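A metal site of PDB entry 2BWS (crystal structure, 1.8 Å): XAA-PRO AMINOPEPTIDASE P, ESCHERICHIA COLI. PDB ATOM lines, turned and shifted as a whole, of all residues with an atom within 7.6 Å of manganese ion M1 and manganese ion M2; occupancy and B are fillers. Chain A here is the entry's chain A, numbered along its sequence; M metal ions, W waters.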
ATOM      1  N   TYR A 229       9.493   1.599 -17.739  1.00  0.00           N
ATOM      2  CA  TYR A 229       9.409   0.635 -16.633  1.00  0.00           C
ATOM      3  C   TYR A 229       8.942   1.416 -15.410  1.00  0.00           C
ATOM      4  O   TYR A 229       8.972   2.639 -15.409  1.00  0.00           O
ATOM      5  CB  TYR A 229      10.752  -0.025 -16.321  1.00  0.00           C
ATOM      6  CG  TYR A 229      11.874   0.944 -16.110  1.00  0.00           C
ATOM      7  CD1 TYR A 229      12.586   1.469 -17.181  1.00  0.00           C
ATOM      8  CD2 TYR A 229      12.211   1.401 -14.818  1.00  0.00           C
ATOM      9  CE1 TYR A 229      13.594   2.392 -17.015  1.00  0.00           C
ATOM     10  CE2 TYR A 229      13.254   2.333 -14.631  1.00  0.00           C
ATOM     11  CZ  TYR A 229      13.935   2.826 -15.733  1.00  0.00           C
ATOM     12  OH  TYR A 229      14.959   3.735 -15.592  1.00  0.00           O
ATOM     13  N   ILE A 232      11.450   3.941  -9.874  1.00  0.00           N
ATOM     14  CA  ILE A 232      12.012   3.586  -8.572  1.00  0.00           C
ATOM     15  C   ILE A 232      12.495   4.895  -7.936  1.00  0.00           C
ATOM     16  O   ILE A 232      13.320   5.601  -8.519  1.00  0.00           O
ATOM     17  CB  ILE A 232      13.209   2.633  -8.763  1.00  0.00           C
ATOM     18  CG1 ILE A 232      12.738   1.283  -9.311  1.00  0.00           C
ATOM     19  CG2 ILE A 232      14.031   2.505  -7.490  1.00  0.00           C
ATOM     20  CD1 ILE A 232      13.751   0.558 -10.148  1.00  0.00           C
ATOM     21  N   LEU A 242      16.613  -3.089  -4.897  1.00  0.00           N
ATOM     22  CA  LEU A 242      17.015  -2.775  -6.269  1.00  0.00           C
ATOM     23  C   LEU A 242      15.914  -2.174  -7.166  1.00  0.00           C
ATOM     24  O   LEU A 242      16.154  -1.175  -7.876  1.00  0.00           O
ATOM     25  CB  LEU A 242      17.617  -4.029  -6.940  1.00  0.00           C
ATOM     26  CG  LEU A 242      18.940  -4.468  -6.300  1.00  0.00           C
ATOM     27  CD1 LEU A 242      19.530  -5.632  -7.077  1.00  0.00           C
ATOM     28  CD2 LEU A 242      19.958  -3.312  -6.210  1.00  0.00           C
ATOM     29  N   ILE A 259      17.064   7.325  -7.691  1.00  0.00           N
ATOM     30  CA  ILE A 259      15.993   7.377  -8.668  1.00  0.00           C
ATOM     31  C   ILE A 259      16.428   6.625  -9.926  1.00  0.00           C
ATOM     32  O   ILE A 259      17.429   6.997 -10.550  1.00  0.00           O
ATOM     33  CB  ILE A 259      15.611   8.804  -9.028  1.00  0.00           C
ATOM     34  CG1 ILE A 259      15.188   9.578  -7.774  1.00  0.00           C
ATOM     35  CG2 ILE A 259      14.498   8.807 -10.062  1.00  0.00           C
ATOM     36  CD1 ILE A 259      14.645  10.975  -8.069  1.00  0.00           C
ATOM     37  N   ASP A 260      15.674   5.581 -10.252  1.00  0.00           N
ATOM     38  CA  ASP A 260      15.875   4.812 -11.480  1.00  0.00           C
ATOM     39  C   ASP A 260      14.585   4.985 -12.274  1.00  0.00           C
ATOM     40  O   ASP A 260      13.527   4.518 -11.864  1.00  0.00           O
ATOM     41  CB  ASP A 260      16.163   3.352 -11.160  1.00  0.00           C
ATOM     42  CG  ASP A 260      16.688   2.560 -12.378  1.00  0.00           C
ATOM     43  OD1 ASP A 260      16.521   2.990 -13.543  1.00  0.00           O
ATOM     44  OD2 ASP A 260      17.299   1.488 -12.147  1.00  0.00           O
ATOM     45  N   ALA A 261      14.659   5.768 -13.351  1.00  0.00           N
ATOM     46  CA  ALA A 261      13.499   6.088 -14.177  1.00  0.00           C
ATOM     47  C   ALA A 261      13.907   6.316 -15.610  1.00  0.00           C
ATOM     48  O   ALA A 261      15.003   6.856 -15.896  1.00  0.00           O
ATOM     49  CB  ALA A 261      12.770   7.333 -13.653  1.00  0.00           C
ATOM     50  N   GLY A 262      13.011   5.943 -16.522  1.00  0.00           N
ATOM     51  CA  GLY A 262      13.234   6.117 -17.944  1.00  0.00           C
ATOM     52  C   GLY A 262      11.940   6.265 -18.710  1.00  0.00           C
ATOM     53  O   GLY A 262      10.915   5.676 -18.361  1.00  0.00           O
ATOM     54  N   GLY A 270      14.551   4.943 -22.513  1.00  0.00           N
ATOM     55  CA  GLY A 270      15.617   5.531 -21.726  1.00  0.00           C
ATOM     56  C   GLY A 270      15.684   4.790 -20.400  1.00  0.00           C
ATOM     57  O   GLY A 270      14.724   4.097 -20.004  1.00  0.00           O
ATOM     58  N   ASP A 271      16.813   4.900 -19.721  1.00  0.00           N
ATOM     59  CA  ASP A 271      17.025   4.196 -18.462  1.00  0.00           C
ATOM     60  C   ASP A 271      18.170   4.880 -17.714  1.00  0.00           C
ATOM     61  O   ASP A 271      19.343   4.594 -17.956  1.00  0.00           O
ATOM     62  CB  ASP A 271      17.320   2.723 -18.746  1.00  0.00           C
ATOM     63  CG  ASP A 271      17.550   1.897 -17.489  1.00  0.00           C
ATOM     64  OD1 ASP A 271      17.420   2.380 -16.344  1.00  0.00           O
ATOM     65  OD2 ASP A 271      17.868   0.698 -17.663  1.00  0.00           O
ATOM     66  N   ILE A 272      17.832   5.779 -16.800  1.00  0.00           N
ATOM     67  CA  ILE A 272      18.835   6.499 -16.029  1.00  0.00           C
ATOM     68  C   ILE A 272      18.633   6.227 -14.549  1.00  0.00           C
ATOM     69  O   ILE A 272      17.481   6.160 -14.089  1.00  0.00           O
ATOM     70  CB  ILE A 272      18.758   8.033 -16.291  1.00  0.00           C
ATOM     71  CG1 ILE A 272      19.190   8.390 -17.721  1.00  0.00           C
ATOM     72  CG2 ILE A 272      19.586   8.815 -15.257  1.00  0.00           C
ATOM     73  CD1 ILE A 272      19.067   9.852 -18.042  1.00  0.00           C
ATOM     74  N   THR A 273      19.744   6.064 -13.830  1.00  0.00           N
ATOM     75  CA  THR A 273      19.738   6.116 -12.366  1.00  0.00           C
ATOM     76  C   THR A 273      20.650   7.242 -11.906  1.00  0.00           C
ATOM     77  O   THR A 273      21.790   7.393 -12.400  1.00  0.00           O
ATOM     78  CB  THR A 273      20.187   4.805 -11.695  1.00  0.00           C
ATOM     79  OG1 THR A 273      19.482   3.687 -12.257  1.00  0.00           O
ATOM     80  CG2 THR A 273      19.934   4.875 -10.173  1.00  0.00           C
ATOM     81  N   GLY A 351      24.310  -7.126 -12.523  1.00  0.00           N
ATOM     82  CA  GLY A 351      25.172  -6.897 -13.678  1.00  0.00           C
ATOM     83  C   GLY A 351      25.482  -5.422 -13.892  1.00  0.00           C
ATOM     84  O   GLY A 351      24.714  -4.535 -13.476  1.00  0.00           O
ATOM     85  N   LEU A 352      26.614  -5.158 -14.531  1.00  0.00           N
ATOM     86  CA  LEU A 352      27.028  -3.804 -14.846  1.00  0.00           C
ATOM     87  C   LEU A 352      26.217  -3.172 -15.991  1.00  0.00           C
ATOM     88  O   LEU A 352      26.026  -1.949 -16.034  1.00  0.00           O
ATOM     89  CB  LEU A 352      28.517  -3.797 -15.238  1.00  0.00           C
ATOM     90  CG  LEU A 352      29.166  -2.442 -15.565  1.00  0.00           C
ATOM     91  CD1 LEU A 352      29.134  -1.506 -14.344  1.00  0.00           C
ATOM     92  CD2 LEU A 352      30.597  -2.673 -16.062  1.00  0.00           C
ATOM     93  N   SER A 353      25.783  -4.010 -16.925  1.00  0.00           N
ATOM     94  CA  SER A 353      25.247  -3.540 -18.192  1.00  0.00           C
ATOM     95  C   SER A 353      24.217  -4.489 -18.758  1.00  0.00           C
ATOM     96  O   SER A 353      24.428  -5.697 -18.753  1.00  0.00           O
ATOM     97  CB  SER A 353      26.385  -3.398 -19.211  1.00  0.00           C
ATOM     98  OG  SER A 353      27.276  -2.369 -18.854  1.00  0.00           O
ATOM     99  N   HIS A 354      23.133  -3.927 -19.270  1.00  0.00           N
ATOM    100  CA  HIS A 354      22.192  -4.680 -20.091  1.00  0.00           C
ATOM    101  C   HIS A 354      21.943  -3.921 -21.406  1.00  0.00           C
ATOM    102  O   HIS A 354      22.081  -2.699 -21.480  1.00  0.00           O
ATOM    103  CB  HIS A 354      20.875  -4.957 -19.340  1.00  0.00           C
ATOM    104  CG  HIS A 354      20.170  -3.721 -18.878  1.00  0.00           C
ATOM    105  ND1 HIS A 354      19.395  -2.957 -19.717  1.00  0.00           N
ATOM    106  CD2 HIS A 354      20.135  -3.108 -17.670  1.00  0.00           C
ATOM    107  CE1 HIS A 354      18.909  -1.913 -19.041  1.00  0.00           C
ATOM    108  NE2 HIS A 354      19.358  -1.978 -17.803  1.00  0.00           N
ATOM    109  N   TRP A 355      21.597  -4.676 -22.441  1.00  0.00           N
ATOM    110  CA  TRP A 355      21.160  -4.100 -23.712  1.00  0.00           C
ATOM    111  C   TRP A 355      19.947  -3.191 -23.477  1.00  0.00           C
ATOM    112  O   TRP A 355      19.156  -3.404 -22.538  1.00  0.00           O
ATOM    113  CB  TRP A 355      20.738  -5.169 -24.721  1.00  0.00           C
ATOM    114  CG  TRP A 355      21.693  -6.323 -24.965  1.00  0.00           C
ATOM    115  CD1 TRP A 355      21.370  -7.643 -24.936  1.00  0.00           C
ATOM    116  CD2 TRP A 355      23.093  -6.247 -25.310  1.00  0.00           C
ATOM    117  NE1 TRP A 355      22.484  -8.412 -25.226  1.00  0.00           N
ATOM    118  CE2 TRP A 355      23.553  -7.588 -25.470  1.00  0.00           C
ATOM    119  CE3 TRP A 355      23.993  -5.202 -25.513  1.00  0.00           C
ATOM    120  CZ2 TRP A 355      24.873  -7.897 -25.818  1.00  0.00           C
ATOM    121  CZ3 TRP A 355      25.321  -5.517 -25.852  1.00  0.00           C
ATOM    122  CH2 TRP A 355      25.745  -6.852 -26.007  1.00  0.00           C
ATOM    123  N   LEU A 356      19.804  -2.201 -24.359  1.00  0.00           N
ATOM    124  CA  LEU A 356      18.718  -1.220 -24.257  1.00  0.00           C
ATOM    125  C   LEU A 356      18.087  -1.025 -25.637  1.00  0.00           C
ATOM    126  O   LEU A 356      18.799  -0.943 -26.652  1.00  0.00           O
ATOM    127  CB  LEU A 356      19.294   0.097 -23.741  1.00  0.00           C
ATOM    128  CG  LEU A 356      18.326   1.241 -23.437  1.00  0.00           C
ATOM    129  CD1 LEU A 356      17.456   0.909 -22.224  1.00  0.00           C
ATOM    130  CD2 LEU A 356      19.100   2.536 -23.205  1.00  0.00           C
ATOM    131  N   VAL A 360      13.509  -2.137 -22.050  1.00  0.00           N
ATOM    132  CA  VAL A 360      14.549  -1.629 -21.183  1.00  0.00           C
ATOM    133  C   VAL A 360      15.631  -2.694 -20.950  1.00  0.00           C
ATOM    134  O   VAL A 360      16.814  -2.373 -21.014  1.00  0.00           O
ATOM    135  CB  VAL A 360      14.006  -1.019 -19.842  1.00  0.00           C
ATOM    136  CG1 VAL A 360      13.230  -2.021 -19.029  1.00  0.00           C
ATOM    137  CG2 VAL A 360      15.141  -0.418 -19.040  1.00  0.00           C
ATOM    138  N   HIS A 361      15.222  -3.931 -20.666  1.00  0.00           N
ATOM    139  CA  HIS A 361      16.148  -5.051 -20.681  1.00  0.00           C
ATOM    140  C   HIS A 361      16.052  -5.687 -22.056  1.00  0.00           C
ATOM    141  O   HIS A 361      15.244  -6.598 -22.304  1.00  0.00           O
ATOM    142  CB  HIS A 361      15.856  -6.058 -19.588  1.00  0.00           C
ATOM    143  CG  HIS A 361      16.016  -5.516 -18.213  1.00  0.00           C
ATOM    144  ND1 HIS A 361      15.369  -6.050 -17.130  1.00  0.00           N
ATOM    145  CD2 HIS A 361      16.722  -4.449 -17.748  1.00  0.00           C
ATOM    146  CE1 HIS A 361      15.689  -5.361 -16.046  1.00  0.00           C
ATOM    147  NE2 HIS A 361      16.507  -4.378 -16.391  1.00  0.00           N
ATOM    148  N   LEU A 380      23.611  -0.096 -24.741  1.00  0.00           N
ATOM    149  CA  LEU A 380      23.623  -0.747 -23.435  1.00  0.00           C
ATOM    150  C   LEU A 380      23.685   0.283 -22.323  1.00  0.00           C
ATOM    151  O   LEU A 380      24.048   1.443 -22.549  1.00  0.00           O
ATOM    152  CB  LEU A 380      24.780  -1.739 -23.301  1.00  0.00           C
ATOM    153  CG  LEU A 380      26.244  -1.233 -23.457  1.00  0.00           C
ATOM    154  CD1 LEU A 380      27.243  -2.062 -22.640  1.00  0.00           C
ATOM    155  CD2 LEU A 380      26.659  -1.197 -24.930  1.00  0.00           C
ATOM    156  N   THR A 381      23.310  -0.158 -21.134  1.00  0.00           N
ATOM    157  CA  THR A 381      23.438   0.661 -19.940  1.00  0.00           C
ATOM    158  C   THR A 381      24.763   0.401 -19.235  1.00  0.00           C
ATOM    159  O   THR A 381      25.418  -0.601 -19.487  1.00  0.00           O
ATOM    160  CB  THR A 381      22.297   0.389 -18.945  1.00  0.00           C
ATOM    161  OG1 THR A 381      22.436  -0.944 -18.411  1.00  0.00           O
ATOM    162  CG2 THR A 381      20.943   0.555 -19.631  1.00  0.00           C
ATOM    163  N   VAL A 382      25.145   1.312 -18.361  1.00  0.00           N
ATOM    164  CA  VAL A 382      26.299   1.136 -17.492  1.00  0.00           C
ATOM    165  C   VAL A 382      25.850   1.591 -16.115  1.00  0.00           C
ATOM    166  O   VAL A 382      25.556   2.768 -15.915  1.00  0.00           O
ATOM    167  CB  VAL A 382      27.517   1.982 -17.974  1.00  0.00           C
ATOM    168  CG1 VAL A 382      28.765   1.654 -17.201  1.00  0.00           C
ATOM    169  CG2 VAL A 382      27.736   1.793 -19.495  1.00  0.00           C
ATOM    170  N   GLU A 383      25.701   0.640 -15.195  1.00  0.00           N
ATOM    171  CA  GLU A 383      25.001   0.909 -13.941  1.00  0.00           C
ATOM    172  C   GLU A 383      25.615   0.246 -12.710  1.00  0.00           C
ATOM    173  O   GLU A 383      24.976  -0.567 -12.025  1.00  0.00           O
ATOM    174  CB  GLU A 383      23.518   0.545 -14.074  1.00  0.00           C
ATOM    175  CG  GLU A 383      23.192  -0.883 -14.406  1.00  0.00           C
ATOM    176  CD  GLU A 383      21.693  -1.025 -14.644  1.00  0.00           C
ATOM    177  OE1 GLU A 383      20.908  -0.743 -13.714  1.00  0.00           O
ATOM    178  OE2 GLU A 383      21.317  -1.320 -15.783  1.00  0.00           O
ATOM    179  N   ARG A 404      23.305   3.855  -6.848  1.00  0.00           N
ATOM    180  CA  ARG A 404      23.521   3.428  -8.225  1.00  0.00           C
ATOM    181  C   ARG A 404      23.581   4.649  -9.126  1.00  0.00           C
ATOM    182  O   ARG A 404      22.884   5.649  -8.904  1.00  0.00           O
ATOM    183  CB  ARG A 404      22.424   2.446  -8.657  1.00  0.00           C
ATOM    184  CG  ARG A 404      22.483   2.029 -10.129  1.00  0.00           C
ATOM    185  CD  ARG A 404      21.629   0.796 -10.449  1.00  0.00           C
ATOM    186  NE  ARG A 404      20.166   1.025 -10.380  1.00  0.00           N
ATOM    187  CZ  ARG A 404      19.379   0.672  -9.369  1.00  0.00           C
ATOM    188  NH1 ARG A 404      19.859   0.107  -8.272  1.00  0.00           N
ATOM    189  NH2 ARG A 404      18.060   0.902  -9.439  1.00  0.00           N
ATOM    190  N   GLU A 406      23.709   5.395 -13.336  1.00  0.00           N
ATOM    191  CA  GLU A 406      23.490   4.664 -14.588  1.00  0.00           C
ATOM    192  C   GLU A 406      23.328   5.609 -15.765  1.00  0.00           C
ATOM    193  O   GLU A 406      22.474   6.515 -15.732  1.00  0.00           O
ATOM    194  CB  GLU A 406      22.263   3.761 -14.463  1.00  0.00           C
ATOM    195  CG  GLU A 406      21.748   3.202 -15.776  1.00  0.00           C
ATOM    196  CD  GLU A 406      20.575   2.261 -15.576  1.00  0.00           C
ATOM    197  OE1 GLU A 406      19.782   2.451 -14.635  1.00  0.00           O
ATOM    198  OE2 GLU A 406      20.423   1.333 -16.395  1.00  0.00           O
ATOM    199  N   ASP A 407      24.092   5.329 -16.819  1.00  0.00           N
ATOM    200  CA  ASP A 407      23.996   6.021 -18.115  1.00  0.00           C
ATOM    201  C   ASP A 407      23.675   4.999 -19.209  1.00  0.00           C
ATOM    202  O   ASP A 407      23.896   3.809 -19.034  1.00  0.00           O
ATOM    203  CB  ASP A 407      25.310   6.738 -18.443  1.00  0.00           C
ATOM    204  CG  ASP A 407      25.457   8.092 -17.757  1.00  0.00           C
ATOM    205  OD1 ASP A 407      24.437   8.750 -17.419  1.00  0.00           O
ATOM    206  OD2 ASP A 407      26.610   8.507 -17.552  1.00  0.00           O
ATOM    207  N   ASP A 408      23.176   5.504 -20.337  1.00  0.00           N
ATOM    208  CA  ASP A 408      22.899   4.726 -21.531  1.00  0.00           C
ATOM    209  C   ASP A 408      23.898   5.138 -22.596  1.00  0.00           C
ATOM    210  O   ASP A 408      24.105   6.336 -22.829  1.00  0.00           O
ATOM    211  CB  ASP A 408      21.474   4.972 -22.035  1.00  0.00           C
ATOM    212  CG  ASP A 408      20.439   4.800 -20.933  1.00  0.00           C
ATOM    213  OD1 ASP A 408      20.673   3.971 -20.037  1.00  0.00           O
ATOM    214  OD2 ASP A 408      19.389   5.493 -20.994  1.00  0.00           O
HETATM  215 MN    MN M   1      19.320  -0.373 -16.395  1.00  0.00          MN
HETATM  216 MN    MN M   2      17.862   1.589 -14.531  1.00  0.00          MN
HETATM  217  O   HOH W   1      15.884   0.312 -14.740  1.00  0.00           O
HETATM  218  O   HOH W   2      18.571  -0.283 -14.687  1.00  0.00           O
HETATM  219  O   HOH W   3      17.365  -2.524 -14.559  1.00  0.00           O
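Manganese ion M1 is bound by water W2, the side-chain carboxylate (OE2) of Glu 406, a ring nitrogen (NE2) of His 354, the side-chain carboxylate (OD2) of Asp 271 and the side-chain carboxylate (OE2) of Glu 383.
Manganese ion M1 has five donor atoms within binding distance.
The side-chain hydroxyl (OH) of Tyr 229 sits close to the side-chain carboxylate (OD1) of Asp 271, at 2.9 Å.
The backbone carbonyl oxygen of His 354 is in hydrogen-bond range of the backbone NH of Thr 381.
The backbone carbonyl oxygen of Val 360 sits close to a ring nitrogen (ND1) of His 354 (2.9 Å).
NH2 of Arg 404 sits close to OD2 of Asp 260, at 2.9 Å.
The backbone carbonyl oxygen (O) of Ile 232 sits at hydrogen-bond distance from the backbone NH (N) of Asp 260 (2.9 Å).
The side-chain hydroxyl of Thr 381 lies close to the side-chain carboxylate of Glu 383 (2.9 Å).
O of Leu 352 sits at hydrogen-bond distance from N of Glu 383.
N of Gly 262 is in hydrogen-bond range of OH of Tyr 229 (3.1 Å).
Merely in contact with manganese ion M1: Thr 381 (3.7 Å).
The nearest printed residue that does not touch manganese ion M1 is His 361 (4.9 Å).
Manganese ion M2 is bound by water W2, at 2.0 Å.
Manganese ion M2 is bound by OD1 of Asp 271, 2.0 Å away.
Manganese ion M2 is bound by the side-chain carboxylate (OE1) of Glu 406 (2.1 Å).
The side-chain carboxylate (OD1) of Asp 260 binds manganese ion M2 (2.2 Å).
Manganese ion M2 is bound by water W1.
Manganese ion M2 is bound by OD2 of Asp 260, 2.5 Å away.
Tyr 229 touches manganese ion M2 (OH to MN, 3.8 Å).
Thr 273 touches manganese ion M2 (OG1 to MN, 3.5 Å).
Of the 27 residues printed, 6 come within 4 Å of manganese ion M2.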
